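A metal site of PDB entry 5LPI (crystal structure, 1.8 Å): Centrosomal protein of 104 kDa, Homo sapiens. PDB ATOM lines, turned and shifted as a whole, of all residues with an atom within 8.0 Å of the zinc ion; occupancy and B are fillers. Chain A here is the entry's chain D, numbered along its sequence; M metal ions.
Within 4 Å of the zinc ion: Cys 104, Cys 107, His 121 and Cys 128.
The nearest printed residue that does not touch the zinc ion is Leu 106 (4.5 Å).
The side-chain sulfur (SG) of Cys 128 lies close to the backbone NH (N) of Met 130 (3.4 Å).
O of Cys 128 sits at hydrogen-bond distance from NZ of Lys 134, at 3.1 Å.
The backbone NH (N) of Leu 106 sits close to the side-chain sulfur (SG) of Cys 104, 3.4 Å away.
N of Cys 104 sits at hydrogen-bond distance from O of Glu 109 (2.9 Å).
SG of Cys 107 lies close to N of Glu 109, at 3.8 Å.
The zinc ion is bound by NE2 of His 121, SG of Cys 128, SG of Cys 104 and SG of Cys 107.
The zinc ion has four donor atoms within binding distance.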
ATOM      1  N   ILE A  51      -3.403  -0.994  24.377  1.00  0.00           N
ATOM      2  CA  ILE A  51      -3.792  -2.286  24.951  1.00  0.00           C
ATOM      3  C   ILE A  51      -4.223  -2.109  26.401  1.00  0.00           C
ATOM      4  O   ILE A  51      -5.213  -2.706  26.844  1.00  0.00           O
ATOM      5  CB  ILE A  51      -2.640  -3.303  24.817  1.00  0.00           C
ATOM      6  CG1 ILE A  51      -2.394  -3.600  23.329  1.00  0.00           C
ATOM      7  CG2 ILE A  51      -2.966  -4.600  25.568  1.00  0.00           C
ATOM      8  CD1 ILE A  51      -1.117  -4.348  23.068  1.00  0.00           C
ATOM      9  N   ARG A 103      -4.392  -5.663  34.477  1.00  0.00           N
ATOM     10  CA  ARG A 103      -5.085  -6.784  33.865  1.00  0.00           C
ATOM     11  C   ARG A 103      -4.871  -6.728  32.358  1.00  0.00           C
ATOM     12  O   ARG A 103      -5.296  -5.776  31.708  1.00  0.00           O
ATOM     13  CB  ARG A 103      -6.581  -6.758  34.186  1.00  0.00           C
ATOM     14  CG  ARG A 103      -7.427  -7.664  33.313  1.00  0.00           C
ATOM     15  CD  ARG A 103      -6.999  -9.118  33.437  1.00  0.00           C
ATOM     16  NE  ARG A 103      -8.016 -10.045  32.963  1.00  0.00           N
ATOM     17  CZ  ARG A 103      -8.681 -10.904  33.741  1.00  0.00           C
ATOM     18  NH1 ARG A 103      -8.419 -10.970  35.046  1.00  0.00           N
ATOM     19  NH2 ARG A 103      -9.578 -11.729  33.207  1.00  0.00           N
ATOM     20  N   CYS A 104      -4.207  -7.752  31.821  1.00  0.00           N
ATOM     21  CA  CYS A 104      -3.990  -7.808  30.374  1.00  0.00           C
ATOM     22  C   CYS A 104      -5.258  -8.308  29.698  1.00  0.00           C
ATOM     23  O   CYS A 104      -5.700  -9.420  29.998  1.00  0.00           O
ATOM     24  CB  CYS A 104      -2.833  -8.722  30.002  1.00  0.00           C
ATOM     25  SG  CYS A 104      -2.523  -8.650  28.208  1.00  0.00           S
ATOM     26  N   PRO A 105      -5.858  -7.539  28.794  1.00  0.00           N
ATOM     27  CA  PRO A 105      -7.042  -8.025  28.081  1.00  0.00           C
ATOM     28  C   PRO A 105      -6.711  -9.020  26.976  1.00  0.00           C
ATOM     29  O   PRO A 105      -7.634  -9.624  26.411  1.00  0.00           O
ATOM     30  CB  PRO A 105      -7.633  -6.746  27.499  1.00  0.00           C
ATOM     31  CG  PRO A 105      -6.388  -5.940  27.127  1.00  0.00           C
ATOM     32  CD  PRO A 105      -5.421  -6.211  28.295  1.00  0.00           C
ATOM     33  N   LEU A 106      -5.437  -9.210  26.634  1.00  0.00           N
ATOM     34  CA  LEU A 106      -5.063 -10.137  25.572  1.00  0.00           C
ATOM     35  C   LEU A 106      -4.836 -11.549  26.102  1.00  0.00           C
ATOM     36  O   LEU A 106      -5.288 -12.526  25.500  1.00  0.00           O
ATOM     37  CB  LEU A 106      -3.815  -9.643  24.842  1.00  0.00           C
ATOM     38  CG  LEU A 106      -3.873  -8.216  24.287  1.00  0.00           C
ATOM     39  CD1 LEU A 106      -2.562  -7.886  23.565  1.00  0.00           C
ATOM     40  CD2 LEU A 106      -5.093  -8.037  23.354  1.00  0.00           C
ATOM     41  N   CYS A 107      -4.125 -11.691  27.222  1.00  0.00           N
ATOM     42  CA  CYS A 107      -3.866 -13.004  27.797  1.00  0.00           C
ATOM     43  C   CYS A 107      -4.590 -13.224  29.115  1.00  0.00           C
ATOM     44  O   CYS A 107      -4.483 -14.325  29.686  1.00  0.00           O
ATOM     45  CB  CYS A 107      -2.352 -13.214  27.984  1.00  0.00           C
ATOM     46  SG  CYS A 107      -1.607 -12.244  29.332  1.00  0.00           S
ATOM     47  N   HIS A 108      -5.298 -12.213  29.637  1.00  0.00           N
ATOM     48  CA  HIS A 108      -6.144 -12.344  30.829  1.00  0.00           C
ATOM     49  C   HIS A 108      -5.351 -12.523  32.123  1.00  0.00           C
ATOM     50  O   HIS A 108      -5.911 -13.014  33.111  1.00  0.00           O
ATOM     51  CB  HIS A 108      -7.147 -13.485  30.682  1.00  0.00           C
ATOM     52  CG  HIS A 108      -7.790 -13.533  29.335  1.00  0.00           C
ATOM     53  ND1 HIS A 108      -8.704 -12.580  28.919  1.00  0.00           N
ATOM     54  CD2 HIS A 108      -7.616 -14.376  28.294  1.00  0.00           C
ATOM     55  CE1 HIS A 108      -9.084 -12.863  27.693  1.00  0.00           C
ATOM     56  NE2 HIS A 108      -8.441 -13.934  27.285  1.00  0.00           N
ATOM     57  N   GLU A 109      -4.090 -12.118  32.178  1.00  0.00           N
ATOM     58  CA  GLU A 109      -3.313 -12.223  33.402  1.00  0.00           C
ATOM     59  C   GLU A 109      -3.431 -10.954  34.232  1.00  0.00           C
ATOM     60  O   GLU A 109      -3.512  -9.840  33.681  1.00  0.00           O
ATOM     61  CB  GLU A 109      -1.849 -12.530  33.086  1.00  0.00           C
ATOM     62  CG  GLU A 109      -1.674 -13.869  32.370  1.00  0.00           C
ATOM     63  CD  GLU A 109      -0.234 -14.168  31.998  1.00  0.00           C
ATOM     64  OE1 GLU A 109       0.666 -13.342  32.284  1.00  0.00           O
ATOM     65  OE2 GLU A 109      -0.016 -15.255  31.406  1.00  0.00           O
ATOM     66  N   ASN A 110      -3.487 -11.123  35.547  1.00  0.00           N
ATOM     67  CA  ASN A 110      -3.351 -10.036  36.496  1.00  0.00           C
ATOM     68  C   ASN A 110      -1.898  -9.981  36.933  1.00  0.00           C
ATOM     69  O   ASN A 110      -1.283 -11.018  37.220  1.00  0.00           O
ATOM     70  CB  ASN A 110      -4.263 -10.223  37.718  1.00  0.00           C
ATOM     71  CG  ASN A 110      -5.760 -10.381  37.356  1.00  0.00           C
ATOM     72  OD1 ASN A 110      -6.320  -9.590  36.579  1.00  0.00           O
ATOM     73  ND2 ASN A 110      -6.401 -11.393  37.939  1.00  0.00           N
ATOM     74  N   PHE A 111      -1.320  -8.786  36.982  1.00  0.00           N
ATOM     75  CA  PHE A 111       0.082  -8.692  37.335  1.00  0.00           C
ATOM     76  C   PHE A 111       0.334  -7.337  37.987  1.00  0.00           C
ATOM     77  O   PHE A 111      -0.583  -6.527  38.118  1.00  0.00           O
ATOM     78  CB  PHE A 111       0.961  -8.945  36.121  1.00  0.00           C
ATOM     79  CG  PHE A 111       0.724  -7.996  34.973  1.00  0.00           C
ATOM     80  CD1 PHE A 111      -0.344  -8.189  34.089  1.00  0.00           C
ATOM     81  CD2 PHE A 111       1.570  -6.925  34.769  1.00  0.00           C
ATOM     82  CE1 PHE A 111      -0.550  -7.320  33.026  1.00  0.00           C
ATOM     83  CE2 PHE A 111       1.372  -6.044  33.697  1.00  0.00           C
ATOM     84  CZ  PHE A 111       0.305  -6.250  32.820  1.00  0.00           C
ATOM     85  N   TRP A 118       3.219  -2.536  32.773  1.00  0.00           N
ATOM     86  CA  TRP A 118       2.583  -2.668  31.461  1.00  0.00           C
ATOM     87  C   TRP A 118       3.624  -2.842  30.362  1.00  0.00           C
ATOM     88  O   TRP A 118       3.513  -3.741  29.511  1.00  0.00           O
ATOM     89  CB  TRP A 118       1.710  -1.460  31.160  1.00  0.00           C
ATOM     90  CG  TRP A 118       0.299  -1.609  31.587  1.00  0.00           C
ATOM     91  CD1 TRP A 118      -0.370  -0.842  32.496  1.00  0.00           C
ATOM     92  CD2 TRP A 118      -0.612  -2.603  31.132  1.00  0.00           C
ATOM     93  NE1 TRP A 118      -1.670  -1.299  32.627  1.00  0.00           N
ATOM     94  CE2 TRP A 118      -1.836  -2.380  31.806  1.00  0.00           C
ATOM     95  CE3 TRP A 118      -0.527  -3.649  30.198  1.00  0.00           C
ATOM     96  CZ2 TRP A 118      -2.957  -3.175  31.582  1.00  0.00           C
ATOM     97  CZ3 TRP A 118      -1.655  -4.438  29.989  1.00  0.00           C
ATOM     98  CH2 TRP A 118      -2.846  -4.199  30.670  1.00  0.00           C
ATOM     99  N   HIS A 121       5.337  -6.278  30.605  1.00  0.00           N
ATOM    100  CA  HIS A 121       4.461  -7.354  30.169  1.00  0.00           C
ATOM    101  C   HIS A 121       4.322  -7.392  28.651  1.00  0.00           C
ATOM    102  O   HIS A 121       4.492  -8.444  28.028  1.00  0.00           O
ATOM    103  CB  HIS A 121       3.082  -7.202  30.803  1.00  0.00           C
ATOM    104  CG  HIS A 121       2.133  -8.283  30.404  1.00  0.00           C
ATOM    105  ND1 HIS A 121       2.166  -9.544  30.974  1.00  0.00           N
ATOM    106  CD2 HIS A 121       1.158  -8.322  29.472  1.00  0.00           C
ATOM    107  CE1 HIS A 121       1.233 -10.297  30.418  1.00  0.00           C
ATOM    108  NE2 HIS A 121       0.599  -9.575  29.507  1.00  0.00           N
ATOM    109  N   LEU A 122       4.031  -6.253  28.039  1.00  0.00           N
ATOM    110  CA  LEU A 122       3.690  -6.240  26.618  1.00  0.00           C
ATOM    111  C   LEU A 122       4.923  -6.291  25.717  1.00  0.00           C
ATOM    112  O   LEU A 122       4.847  -6.844  24.612  1.00  0.00           O
ATOM    113  CB  LEU A 122       2.837  -5.013  26.318  1.00  0.00           C
ATOM    114  CG  LEU A 122       1.425  -5.095  26.907  1.00  0.00           C
ATOM    115  CD1 LEU A 122       0.671  -3.792  26.673  1.00  0.00           C
ATOM    116  CD2 LEU A 122       0.642  -6.276  26.308  1.00  0.00           C
ATOM    117  N   GLY A 127       7.265 -12.182  28.116  1.00  0.00           N
ATOM    118  CA  GLY A 127       6.109 -11.510  28.670  1.00  0.00           C
ATOM    119  C   GLY A 127       4.825 -12.028  28.056  1.00  0.00           C
ATOM    120  O   GLY A 127       4.564 -13.241  28.087  1.00  0.00           O
ATOM    121  N   CYS A 128       4.025 -11.131  27.477  1.00  0.00           N
ATOM    122  CA  CYS A 128       2.713 -11.495  26.952  1.00  0.00           C
ATOM    123  C   CYS A 128       2.849 -12.437  25.759  1.00  0.00           C
ATOM    124  O   CYS A 128       3.594 -12.155  24.822  1.00  0.00           O
ATOM    125  CB  CYS A 128       1.938 -10.243  26.545  1.00  0.00           C
ATOM    126  SG  CYS A 128       0.205 -10.602  26.153  1.00  0.00           S
ATOM    127  N   THR A 129       2.118 -13.541  25.796  1.00  0.00           N
ATOM    128  CA  THR A 129       2.113 -14.489  24.699  1.00  0.00           C
ATOM    129  C   THR A 129       1.043 -14.186  23.662  1.00  0.00           C
ATOM    130  O   THR A 129       0.976 -14.880  22.639  1.00  0.00           O
ATOM    131  CB  THR A 129       1.887 -15.906  25.227  1.00  0.00           C
ATOM    132  OG1 THR A 129       0.532 -16.001  25.669  1.00  0.00           O
ATOM    133  CG2 THR A 129       2.804 -16.174  26.398  1.00  0.00           C
ATOM    134  N   MET A 130       0.176 -13.206  23.911  1.00  0.00           N
ATOM    135  CA  MET A 130      -0.958 -12.956  23.033  1.00  0.00           C
ATOM    136  C   MET A 130      -0.847 -11.603  22.329  1.00  0.00           C
ATOM    137  O   MET A 130      -1.836 -11.151  21.750  1.00  0.00           O
ATOM    138  CB  MET A 130      -2.269 -13.047  23.832  1.00  0.00           C
ATOM    139  CG  MET A 130      -2.588 -14.444  24.356  1.00  0.00           C
ATOM    140  SD  MET A 130      -2.728 -15.642  23.007  1.00  0.00           S
ATOM    141  CE  MET A 130      -4.207 -15.054  22.179  1.00  0.00           C
ATOM    142  N   ASN A 131       0.319 -10.965  22.363  1.00  0.00           N
ATOM    143  CA  ASN A 131       0.519  -9.681  21.692  1.00  0.00           C
ATOM    144  C   ASN A 131       0.975  -9.949  20.260  1.00  0.00           C
ATOM    145  O   ASN A 131       2.148 -10.266  20.021  1.00  0.00           O
ATOM    146  CB  ASN A 131       1.544  -8.841  22.458  1.00  0.00           C
ATOM    147  CG  ASN A 131       1.683  -7.444  21.912  1.00  0.00           C
ATOM    148  OD1 ASN A 131       1.046  -7.084  20.919  1.00  0.00           O
ATOM    149  ND2 ASN A 131       2.525  -6.638  22.560  1.00  0.00           N
ATOM    150  N   LYS A 134       4.162  -8.663  18.665  1.00  0.00           N
ATOM    151  CA  LYS A 134       5.427  -9.094  19.239  1.00  0.00           C
ATOM    152  C   LYS A 134       5.943 -10.312  18.481  1.00  0.00           C
ATOM    153  O   LYS A 134       6.935 -10.222  17.768  1.00  0.00           O
ATOM    154  CB  LYS A 134       5.281  -9.395  20.738  1.00  0.00           C
ATOM    155  CG  LYS A 134       6.594  -9.329  21.491  1.00  0.00           C
ATOM    156  CD  LYS A 134       6.413  -9.126  22.997  1.00  0.00           C
ATOM    157  CE  LYS A 134       5.963 -10.399  23.699  1.00  0.00           C
ATOM    158  NZ  LYS A 134       5.985 -10.241  25.197  1.00  0.00           N
HETATM  159 ZN    ZN M   1      -0.831 -10.261  28.165  1.00  0.00          ZN
